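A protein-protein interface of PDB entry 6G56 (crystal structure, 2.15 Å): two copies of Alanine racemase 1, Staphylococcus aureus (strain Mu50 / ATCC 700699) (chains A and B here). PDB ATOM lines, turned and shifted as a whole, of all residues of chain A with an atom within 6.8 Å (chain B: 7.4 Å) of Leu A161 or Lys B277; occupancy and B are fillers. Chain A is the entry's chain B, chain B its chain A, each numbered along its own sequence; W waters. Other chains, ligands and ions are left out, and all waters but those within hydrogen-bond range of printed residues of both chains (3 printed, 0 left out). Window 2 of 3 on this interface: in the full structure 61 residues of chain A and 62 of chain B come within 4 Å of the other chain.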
ATOM      1  N   PRO A 128     -10.683  -1.405  -9.854  1.00  0.00           N
ATOM      2  CA  PRO A 128     -12.130  -1.619  -9.871  1.00  0.00           C
ATOM      3  C   PRO A 128     -12.654  -2.313 -11.106  1.00  0.00           C
ATOM      4  O   PRO A 128     -13.807  -2.753 -11.103  1.00  0.00           O
ATOM      5  CB  PRO A 128     -12.677  -0.185  -9.854  1.00  0.00           C
ATOM      6  CG  PRO A 128     -11.687   0.570 -10.669  1.00  0.00           C
ATOM      7  CD  PRO A 128     -10.343  -0.053 -10.349  1.00  0.00           C
ATOM      8  N   LYS A 153     -10.625  -5.200  -6.490  1.00  0.00           N
ATOM      9  CA  LYS A 153     -11.925  -5.164  -5.847  1.00  0.00           C
ATOM     10  C   LYS A 153     -12.902  -6.019  -6.626  1.00  0.00           C
ATOM     11  O   LYS A 153     -13.083  -5.803  -7.822  1.00  0.00           O
ATOM     12  CB  LYS A 153     -12.473  -3.741  -5.768  1.00  0.00           C
ATOM     13  CG  LYS A 153     -13.617  -3.614  -4.807  1.00  0.00           C
ATOM     14  CD  LYS A 153     -14.022  -2.147  -4.771  1.00  0.00           C
ATOM     15  CE  LYS A 153     -15.230  -1.918  -3.918  1.00  0.00           C
ATOM     16  NZ  LYS A 153     -15.661  -0.498  -4.019  1.00  0.00           N
ATOM     17  N   LEU A 154     -13.536  -6.952  -5.920  1.00  0.00           N
ATOM     18  CA  LEU A 154     -14.553  -7.822  -6.501  1.00  0.00           C
ATOM     19  C   LEU A 154     -15.919  -7.363  -6.076  1.00  0.00           C
ATOM     20  O   LEU A 154     -16.139  -7.019  -4.905  1.00  0.00           O
ATOM     21  CB  LEU A 154     -14.335  -9.274  -6.067  1.00  0.00           C
ATOM     22  CG  LEU A 154     -13.011  -9.918  -6.494  1.00  0.00           C
ATOM     23  CD1 LEU A 154     -12.961 -11.404  -6.109  1.00  0.00           C
ATOM     24  CD2 LEU A 154     -12.797  -9.784  -7.995  1.00  0.00           C
ATOM     25  N   ASP A 155     -16.842  -7.415  -7.029  1.00  0.00           N
ATOM     26  CA  ASP A 155     -18.247  -7.130  -6.796  1.00  0.00           C
ATOM     27  C   ASP A 155     -18.864  -8.495  -6.589  1.00  0.00           C
ATOM     28  O   ASP A 155     -19.087  -9.227  -7.540  1.00  0.00           O
ATOM     29  CB  ASP A 155     -18.909  -6.493  -8.012  1.00  0.00           C
ATOM     30  CG  ASP A 155     -20.445  -6.512  -7.934  1.00  0.00           C
ATOM     31  OD1 ASP A 155     -21.019  -6.892  -6.900  1.00  0.00           O
ATOM     32  OD2 ASP A 155     -21.082  -6.127  -8.918  1.00  0.00           O
ATOM     33  N   GLY A 159     -23.133  -6.219  -3.231  1.00  0.00           N
ATOM     34  CA  GLY A 159     -22.454  -5.011  -2.766  1.00  0.00           C
ATOM     35  C   GLY A 159     -21.951  -3.935  -3.704  1.00  0.00           C
ATOM     36  O   GLY A 159     -22.607  -3.604  -4.678  1.00  0.00           O
ATOM     37  N   ARG A 160     -20.836  -3.304  -3.337  1.00  0.00           N
ATOM     38  CA  ARG A 160     -20.236  -2.245  -4.154  1.00  0.00           C
ATOM     39  C   ARG A 160     -19.699  -2.732  -5.507  1.00  0.00           C
ATOM     40  O   ARG A 160     -19.445  -3.907  -5.711  1.00  0.00           O
ATOM     41  CB  ARG A 160     -19.095  -1.535  -3.397  1.00  0.00           C
ATOM     42  CG  ARG A 160     -19.430  -1.036  -2.004  1.00  0.00           C
ATOM     43  CD  ARG A 160     -20.464   0.076  -2.024  1.00  0.00           C
ATOM     44  NE  ARG A 160     -20.962   0.401  -0.691  1.00  0.00           N
ATOM     45  CZ  ARG A 160     -20.333   1.194   0.168  1.00  0.00           C
ATOM     46  NH1 ARG A 160     -19.177   1.734  -0.164  1.00  0.00           N
ATOM     47  NH2 ARG A 160     -20.853   1.438   1.361  1.00  0.00           N
ATOM     48  N   LEU A 161     -19.518  -1.801  -6.429  1.00  0.00           N
ATOM     49  CA  LEU A 161     -18.971  -2.099  -7.756  1.00  0.00           C
ATOM     50  C   LEU A 161     -17.517  -2.579  -7.708  1.00  0.00           C
ATOM     51  O   LEU A 161     -16.789  -2.267  -6.797  1.00  0.00           O
ATOM     52  CB  LEU A 161     -19.083  -0.886  -8.670  1.00  0.00           C
ATOM     53  CG  LEU A 161     -20.497  -0.473  -9.084  1.00  0.00           C
ATOM     54  CD1 LEU A 161     -20.439   0.813  -9.882  1.00  0.00           C
ATOM     55  CD2 LEU A 161     -21.201  -1.559  -9.875  1.00  0.00           C
ATOM     56  N   GLY A 162     -17.128  -3.294  -8.735  1.00  0.00           N
ATOM     57  CA  GLY A 162     -15.815  -3.951  -8.819  1.00  0.00           C
ATOM     58  C   GLY A 162     -15.900  -4.953  -9.944  1.00  0.00           C
ATOM     59  O   GLY A 162     -16.821  -4.860 -10.736  1.00  0.00           O
ATOM     60  N   ILE A 163     -14.990  -5.917  -9.996  1.00  0.00           N
ATOM     61  CA  ILE A 163     -14.991  -7.014 -10.974  1.00  0.00           C
ATOM     62  C   ILE A 163     -16.061  -8.006 -10.521  1.00  0.00           C
ATOM     63  O   ILE A 163     -15.965  -8.490  -9.405  1.00  0.00           O
ATOM     64  CB  ILE A 163     -13.617  -7.761 -11.002  1.00  0.00           C
ATOM     65  CG1 ILE A 163     -12.410  -6.822 -11.223  1.00  0.00           C
ATOM     66  CG2 ILE A 163     -13.622  -8.869 -12.046  1.00  0.00           C
ATOM     67  CD1 ILE A 163     -12.481  -6.016 -12.485  1.00  0.00           C
ATOM     68  N   LYS A 164     -17.048  -8.313 -11.354  1.00  0.00           N
ATOM     69  CA  LYS A 164     -18.133  -9.233 -10.983  1.00  0.00           C
ATOM     70  C   LYS A 164     -17.954 -10.651 -11.533  1.00  0.00           C
ATOM     71  O   LYS A 164     -18.502 -11.585 -10.968  1.00  0.00           O
ATOM     72  CB  LYS A 164     -19.451  -8.639 -11.469  1.00  0.00           C
ATOM     73  CG  LYS A 164     -20.735  -9.308 -11.017  1.00  0.00           C
ATOM     74  CD  LYS A 164     -21.938  -8.584 -11.625  1.00  0.00           C
ATOM     75  CE  LYS A 164     -23.112  -9.493 -11.992  1.00  0.00           C
ATOM     76  NZ  LYS A 164     -24.145  -9.585 -10.921  1.00  0.00           N
ATOM     77  N   VAL B 273     -17.328  11.224 -13.407  1.00  0.00           N
ATOM     78  CA  VAL B 273     -17.684   9.810 -13.303  1.00  0.00           C
ATOM     79  C   VAL B 273     -16.374   9.026 -13.333  1.00  0.00           C
ATOM     80  O   VAL B 273     -15.564   9.252 -14.205  1.00  0.00           O
ATOM     81  CB  VAL B 273     -18.591   9.374 -14.476  1.00  0.00           C
ATOM     82  CG1 VAL B 273     -18.795   7.859 -14.501  1.00  0.00           C
ATOM     83  CG2 VAL B 273     -19.922  10.102 -14.387  1.00  0.00           C
ATOM     84  N   GLN B 275     -16.475   5.452 -12.857  1.00  0.00           N
ATOM     85  CA  GLN B 275     -16.841   4.098 -13.321  1.00  0.00           C
ATOM     86  C   GLN B 275     -18.332   4.056 -13.705  1.00  0.00           C
ATOM     87  O   GLN B 275     -19.168   4.696 -13.064  1.00  0.00           O
ATOM     88  CB  GLN B 275     -16.540   3.080 -12.204  1.00  0.00           C
ATOM     89  CG  GLN B 275     -16.859   1.608 -12.495  1.00  0.00           C
ATOM     90  CD  GLN B 275     -16.382   0.668 -11.363  1.00  0.00           C
ATOM     91  OE1 GLN B 275     -16.038   1.111 -10.241  1.00  0.00           O
ATOM     92  NE2 GLN B 275     -16.381  -0.638 -11.645  1.00  0.00           N
ATOM     93  N   THR B 276     -18.664   3.306 -14.756  1.00  0.00           N
ATOM     94  CA  THR B 276     -20.060   3.009 -15.121  1.00  0.00           C
ATOM     95  C   THR B 276     -20.267   1.507 -15.084  1.00  0.00           C
ATOM     96  O   THR B 276     -19.348   0.747 -15.357  1.00  0.00           O
ATOM     97  CB  THR B 276     -20.436   3.544 -16.523  1.00  0.00           C
ATOM     98  OG1 THR B 276     -19.512   3.047 -17.496  1.00  0.00           O
ATOM     99  CG2 THR B 276     -20.384   5.073 -16.539  1.00  0.00           C
ATOM    100  N   LYS B 277     -21.465   1.077 -14.705  1.00  0.00           N
ATOM    101  CA  LYS B 277     -21.860  -0.313 -14.869  1.00  0.00           C
ATOM    102  C   LYS B 277     -23.322  -0.371 -15.303  1.00  0.00           C
ATOM    103  O   LYS B 277     -24.104   0.549 -15.009  1.00  0.00           O
ATOM    104  CB  LYS B 277     -21.619  -1.129 -13.586  1.00  0.00           C
ATOM    105  CG  LYS B 277     -22.024  -2.599 -13.723  1.00  0.00           C
ATOM    106  CD  LYS B 277     -21.406  -3.517 -12.671  1.00  0.00           C
ATOM    107  CE  LYS B 277     -21.486  -4.989 -13.076  1.00  0.00           C
ATOM    108  NZ  LYS B 277     -22.893  -5.469 -13.227  1.00  0.00           N
ATOM    109  N   THR B 278     -23.654  -1.446 -16.022  1.00  0.00           N
ATOM    110  CA  THR B 278     -24.990  -1.683 -16.498  1.00  0.00           C
ATOM    111  C   THR B 278     -25.571  -2.855 -15.726  1.00  0.00           C
ATOM    112  O   THR B 278     -25.052  -3.974 -15.787  1.00  0.00           O
ATOM    113  CB  THR B 278     -24.964  -1.980 -18.003  1.00  0.00           C
ATOM    114  OG1 THR B 278     -24.345  -0.872 -18.667  1.00  0.00           O
ATOM    115  CG2 THR B 278     -26.393  -2.198 -18.549  1.00  0.00           C
ATOM    116  N   LEU B 279     -26.657  -2.560 -15.043  1.00  0.00           N
ATOM    117  CA  LEU B 279     -27.358  -3.536 -14.283  1.00  0.00           C
ATOM    118  C   LEU B 279     -28.439  -4.106 -15.174  1.00  0.00           C
ATOM    119  O   LEU B 279     -29.197  -3.376 -15.806  1.00  0.00           O
ATOM    120  CB  LEU B 279     -27.989  -2.885 -13.063  1.00  0.00           C
ATOM    121  CG  LEU B 279     -27.024  -2.388 -11.996  1.00  0.00           C
ATOM    122  CD1 LEU B 279     -27.784  -2.037 -10.735  1.00  0.00           C
ATOM    123  CD2 LEU B 279     -26.005  -3.473 -11.710  1.00  0.00           C
ATOM    124  N   GLN B 280     -28.481  -5.426 -15.257  1.00  0.00           N
ATOM    125  CA  GLN B 280     -29.528  -6.104 -16.017  1.00  0.00           C
ATOM    126  C   GLN B 280     -30.804  -6.191 -15.170  1.00  0.00           C
ATOM    127  O   GLN B 280     -30.785  -5.924 -13.964  1.00  0.00           O
ATOM    128  CB  GLN B 280     -29.073  -7.475 -16.519  1.00  0.00           C
ATOM    129  CG  GLN B 280     -28.109  -7.420 -17.695  1.00  0.00           C
ATOM    130  CD  GLN B 280     -28.482  -6.384 -18.739  1.00  0.00           C
ATOM    131  OE1 GLN B 280     -29.653  -6.104 -18.965  1.00  0.00           O
ATOM    132  NE2 GLN B 280     -27.479  -5.816 -19.386  1.00  0.00           N
ATOM    133  N   GLU B 283     -31.228  -7.095 -11.267  1.00  0.00           N
ATOM    134  CA  GLU B 283     -29.921  -6.947 -10.647  1.00  0.00           C
ATOM    135  C   GLU B 283     -29.811  -5.611  -9.943  1.00  0.00           C
ATOM    136  O   GLU B 283     -30.078  -4.570 -10.520  1.00  0.00           O
ATOM    137  CB  GLU B 283     -28.812  -7.054 -11.692  1.00  0.00           C
ATOM    138  CG  GLU B 283     -27.404  -6.929 -11.133  1.00  0.00           C
ATOM    139  CD  GLU B 283     -26.358  -6.841 -12.226  1.00  0.00           C
ATOM    140  OE1 GLU B 283     -26.733  -6.564 -13.375  1.00  0.00           O
ATOM    141  OE2 GLU B 283     -25.163  -7.043 -11.945  1.00  0.00           O
ATOM    142  N   SER B 284     -29.241  -5.802  -8.756  1.00  0.00           N
ATOM    143  CA  SER B 284     -28.918  -4.843  -7.779  1.00  0.00           C
ATOM    144  C   SER B 284     -27.454  -4.604  -7.397  1.00  0.00           C
ATOM    145  O   SER B 284     -26.558  -5.416  -7.636  1.00  0.00           O
ATOM    146  CB  SER B 284     -29.634  -5.247  -6.501  1.00  0.00           C
ATOM    147  OG  SER B 284     -29.078  -6.441  -5.999  1.00  0.00           O
ATOM    148  N   VAL B 285     -27.255  -3.438  -6.800  1.00  0.00           N
ATOM    149  CA  VAL B 285     -25.994  -3.014  -6.204  1.00  0.00           C
ATOM    150  C   VAL B 285     -26.361  -2.338  -4.882  1.00  0.00           C
ATOM    151  O   VAL B 285     -27.404  -1.695  -4.769  1.00  0.00           O
ATOM    152  CB  VAL B 285     -25.163  -2.064  -7.088  1.00  0.00           C
ATOM    153  CG1 VAL B 285     -24.467  -2.835  -8.194  1.00  0.00           C
ATOM    154  CG2 VAL B 285     -26.018  -0.935  -7.637  1.00  0.00           C
ATOM    155  N   SER B 286     -25.519  -2.483  -3.871  1.00  0.00           N
ATOM    156  CA  SER B 286     -25.823  -1.862  -2.593  1.00  0.00           C
ATOM    157  C   SER B 286     -24.827  -0.794  -2.137  1.00  0.00           C
ATOM    158  O   SER B 286     -23.696  -1.079  -1.753  1.00  0.00           O
ATOM    159  CB  SER B 286     -25.984  -2.930  -1.519  1.00  0.00           C
ATOM    160  OG  SER B 286     -26.209  -2.357  -0.248  1.00  0.00           O
ATOM    161  N   TYR B 287     -25.315   0.434  -2.117  1.00  0.00           N
ATOM    162  CA  TYR B 287     -24.541   1.573  -1.689  1.00  0.00           C
ATOM    163  C   TYR B 287     -25.346   2.119  -0.556  1.00  0.00           C
ATOM    164  O   TYR B 287     -26.151   3.010  -0.703  1.00  0.00           O
ATOM    165  CB  TYR B 287     -24.355   2.578  -2.816  1.00  0.00           C
ATOM    166  CG  TYR B 287     -23.186   2.219  -3.694  1.00  0.00           C
ATOM    167  CD1 TYR B 287     -23.269   1.167  -4.586  1.00  0.00           C
ATOM    168  CD2 TYR B 287     -21.992   2.906  -3.607  1.00  0.00           C
ATOM    169  CE1 TYR B 287     -22.201   0.823  -5.381  1.00  0.00           C
ATOM    170  CE2 TYR B 287     -20.923   2.573  -4.397  1.00  0.00           C
ATOM    171  CZ  TYR B 287     -21.032   1.525  -5.283  1.00  0.00           C
ATOM    172  OH  TYR B 287     -19.982   1.175  -6.080  1.00  0.00           O
ATOM    173  N   THR B 297     -30.652  -0.796 -16.705  1.00  0.00           N
ATOM    174  CA  THR B 297     -30.230   0.576 -16.474  1.00  0.00           C
ATOM    175  C   THR B 297     -28.736   0.758 -16.211  1.00  0.00           C
ATOM    176  O   THR B 297     -28.079  -0.102 -15.637  1.00  0.00           O
ATOM    177  CB  THR B 297     -30.970   1.153 -15.259  1.00  0.00           C
ATOM    178  OG1 THR B 297     -30.357   0.680 -14.059  1.00  0.00           O
ATOM    179  CG2 THR B 297     -32.421   0.736 -15.254  1.00  0.00           C
ATOM    180  N   THR B 298     -28.213   1.903 -16.617  1.00  0.00           N
ATOM    181  CA  THR B 298     -26.806   2.200 -16.388  1.00  0.00           C
ATOM    182  C   THR B 298     -26.664   3.070 -15.142  1.00  0.00           C
ATOM    183  O   THR B 298     -27.450   4.001 -14.930  1.00  0.00           O
ATOM    184  CB  THR B 298     -26.175   2.881 -17.614  1.00  0.00           C
ATOM    185  OG1 THR B 298     -26.204   1.943 -18.701  1.00  0.00           O
ATOM    186  CG2 THR B 298     -24.725   3.259 -17.357  1.00  0.00           C
ATOM    187  N   ILE B 299     -25.664   2.755 -14.314  1.00  0.00           N
ATOM    188  CA  ILE B 299     -25.324   3.603 -13.162  1.00  0.00           C
ATOM    189  C   ILE B 299     -23.907   4.159 -13.287  1.00  0.00           C
ATOM    190  O   ILE B 299     -23.042   3.535 -13.915  1.00  0.00           O
ATOM    191  CB  ILE B 299     -25.542   2.869 -11.823  1.00  0.00           C
ATOM    192  CG1 ILE B 299     -24.567   1.703 -11.644  1.00  0.00           C
ATOM    193  CG2 ILE B 299     -26.994   2.383 -11.729  1.00  0.00           C
ATOM    194  CD1 ILE B 299     -24.535   1.158 -10.231  1.00  0.00           C
ATOM    195  N   ALA B 300     -23.694   5.327 -12.680  1.00  0.00           N
ATOM    196  CA  ALA B 300     -22.392   5.987 -12.640  1.00  0.00           C
ATOM    197  C   ALA B 300     -21.973   6.223 -11.197  1.00  0.00           C
ATOM    198  O   ALA B 300     -22.780   6.607 -10.350  1.00  0.00           O
ATOM    199  CB  ALA B 300     -22.417   7.310 -13.386  1.00  0.00           C
ATOM    200  N   LEU B 301     -20.693   5.986 -10.945  1.00  0.00           N
ATOM    201  CA  LEU B 301     -20.065   6.134  -9.642  1.00  0.00           C
ATOM    202  C   LEU B 301     -19.303   7.473  -9.642  1.00  0.00           C
ATOM    203  O   LEU B 301     -18.448   7.704 -10.502  1.00  0.00           O
ATOM    204  CB  LEU B 301     -19.088   4.985  -9.418  1.00  0.00           C
ATOM    205  CG  LEU B 301     -18.205   4.946  -8.164  1.00  0.00           C
ATOM    206  CD1 LEU B 301     -19.084   4.936  -6.934  1.00  0.00           C
ATOM    207  CD2 LEU B 301     -17.298   3.706  -8.199  1.00  0.00           C
ATOM    208  N   GLN B 336     -18.508   8.118  -1.823  1.00  0.00           N
ATOM    209  CA  GLN B 336     -19.034   7.752  -3.123  1.00  0.00           C
ATOM    210  C   GLN B 336     -20.512   8.006  -3.221  1.00  0.00           C
ATOM    211  O   GLN B 336     -21.257   7.897  -2.251  1.00  0.00           O
ATOM    212  CB  GLN B 336     -18.785   6.275  -3.407  1.00  0.00           C
ATOM    213  CG  GLN B 336     -17.308   5.940  -3.582  1.00  0.00           C
ATOM    214  CD  GLN B 336     -17.073   4.477  -3.902  1.00  0.00           C
ATOM    215  OE1 GLN B 336     -17.765   3.614  -3.397  1.00  0.00           O
ATOM    216  NE2 GLN B 336     -16.094   4.202  -4.745  1.00  0.00           N
ATOM    217  N   ILE B 338     -23.763   7.160  -6.109  1.00  0.00           N
ATOM    218  CA  ILE B 338     -24.186   6.528  -7.351  1.00  0.00           C
ATOM    219  C   ILE B 338     -25.375   7.294  -7.965  1.00  0.00           C
ATOM    220  O   ILE B 338     -26.271   7.798  -7.260  1.00  0.00           O
ATOM    221  CB  ILE B 338     -24.417   5.005  -7.251  1.00  0.00           C
ATOM    222  CG1 ILE B 338     -25.263   4.610  -6.053  1.00  0.00           C
ATOM    223  CG2 ILE B 338     -23.078   4.282  -7.241  1.00  0.00           C
ATOM    224  CD1 ILE B 338     -26.034   3.311  -6.324  1.00  0.00           C
ATOM    225  N   VAL B 339     -25.326   7.390  -9.287  1.00  0.00           N
ATOM    226  CA  VAL B 339     -26.282   8.136 -10.066  1.00  0.00           C
ATOM    227  C   VAL B 339     -26.785   7.289 -11.231  1.00  0.00           C
ATOM    228  O   VAL B 339     -26.003   6.624 -11.907  1.00  0.00           O
ATOM    229  CB  VAL B 339     -25.623   9.410 -10.601  1.00  0.00           C
ATOM    230  CG1 VAL B 339     -26.514  10.136 -11.609  1.00  0.00           C
ATOM    231  CG2 VAL B 339     -25.333  10.339  -9.446  1.00  0.00           C
ATOM    232  N   VAL B 341     -27.900   6.985 -14.907  1.00  0.00           N
ATOM    233  CA  VAL B 341     -27.465   7.792 -16.048  1.00  0.00           C
ATOM    234  C   VAL B 341     -27.856   7.149 -17.355  1.00  0.00           C
ATOM    235  O   VAL B 341     -28.037   5.950 -17.403  1.00  0.00           O
ATOM    236  CB  VAL B 341     -25.932   8.000 -16.068  1.00  0.00           C
ATOM    237  CG1 VAL B 341     -25.496   8.775 -14.849  1.00  0.00           C
ATOM    238  CG2 VAL B 341     -25.167   6.681 -16.165  1.00  0.00           C
ATOM    239  N   VAL B 345     -23.305   7.868 -21.136  1.00  0.00           N
ATOM    240  CA  VAL B 345     -22.435   8.385 -20.089  1.00  0.00           C
ATOM    241  C   VAL B 345     -21.289   7.408 -19.826  1.00  0.00           C
ATOM    242  O   VAL B 345     -21.485   6.196 -19.805  1.00  0.00           O
ATOM    243  CB  VAL B 345     -23.217   8.675 -18.789  1.00  0.00           C
ATOM    244  CG1 VAL B 345     -22.270   8.965 -17.622  1.00  0.00           C
ATOM    245  CG2 VAL B 345     -24.175   9.834 -19.015  1.00  0.00           C
HETATM  246  O   HOH W   1     -14.050   1.858  -5.439  1.00  0.00           O
HETATM  247  O   HOH W   2     -22.087  -2.668  -0.530  1.00  0.00           O
HETATM  248  O   HOH W   3     -17.559   1.437  -5.005  1.00  0.00           O
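NE2 of Gln B275 sits at hydrogen-bond distance from O of Pro A128, at 3.4 Å.
The side-chain amino group (NZ) of Lys A164 lies within salt-bridge range of the side-chain carboxylate (OE2) of Glu B283 (2.9 Å).
The backbone NH (N) of Ser B286 lies within hydrogen-bond range of the backbone carbonyl oxygen (O) of Gly A159 (3.2 Å).
O of Ser B286 lies within hydrogen-bond range of NE of Arg A160 (3.3 Å).
N of Leu A161 sits at hydrogen-bond distance from OH of Tyr B287, at 3.0 Å.
The backbone carbonyl oxygen (O) of Gln B275 is in hydrogen-bond range of the backbone NH (N) of Leu B301.
The side-chain amino group of Lys B277 lies within salt-bridge range of the side-chain carboxylate of Glu B283 (3.0 Å).
The backbone carbonyl oxygen of Lys B277 sits at hydrogen-bond distance from the backbone NH of Ile B299 (2.8 Å).
N of Gln B280 lies within hydrogen-bond range of OE1 of Glu B283 (2.8 Å).
The side-chain amino group (NZ) of Lys A153 lies close to the backbone carbonyl oxygen (O) of Leu A161 (3.5 Å).
Among the printed residues, merely in contact across the chains: Gly A159 with Val B285 (3.8 Å), Arg A160 with Tyr B287 (3.5 Å), Arg A160 with Gln B336 (3.998 Å), Leu A161 with Gln B275 (3.97 Å), Leu A161 with Lys B277 (3.4 Å), Leu A161 with Val B285 (3.9 Å) and Lys A164 with Lys B277 (3.6 Å).
Of chain B, only Gln B275, Lys B277, Val B285 and Tyr B287 come within 4 Å of Leu A161.
Lys B277 touches just these residues of chain A: Leu A161 (3.4 Å) and Lys A164 (3.6 Å).
Printed residues of chain B within 4 Å of Lys A164: Lys B277 (3.6 Å) and Glu B283 (2.9 Å).
Printed residues of chain A within 4 Å of Ser B286: Gly A159 and Arg A160.
Of the printed residues of chain B, Arg A160 touches Ser B286, Tyr B287 and Gln B336.
Printed residues of chain A within 4 Å of Gln B336: Arg A160.
Of the printed residues of chain A, Val B285 touches Gly A159 (3.8 Å) and Leu A161 (3.9 Å).
Ala B300 touches none of the printed residues of chain A.
Leu B301 touches none of the printed residues of chain A.
The nearest residue of chain B that does not touch Leu A161 is Ile B299 (4.1 Å).
Along chain A the printed residues that touch a printed residue of chain B span positions 128 to 164.
Of the 22 printed residues of chain B, 7 touch a printed residue of chain A.
Hydrophobic or aromatic side chains of chain B within 4 Å of the printed part of chain A: Val B285 and Tyr B287.
Along chain B the printed residues that touch a printed residue of chain A span positions 275 to 336.
Among the printed residues, 12 pairs touch across the chains.
Among the printed residues, Asp or Glu carboxylates within 4 Å of a Lys or Arg side-chain nitrogen of the other chain: Lys A164 with Glu B283.
No position is printed for both chains.
Of the 12 pairs that touch across the chains among the printed residues, none has its exchanged pair printed and touching as well.
Water W2 lies within hydrogen-bond range of the backbone carbonyl oxygen of Ser B286 (2.6 Å) and the backbone NH of Arg A160 (3.1 Å).
Water W3 lies within hydrogen-bond range of OH of Tyr B287, OE1 of Gln B336 and NZ of Lys A153.
Water W1 bridges the side-chain amide nitrogen of Gln B336 and the side-chain amino group of Lys A153.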
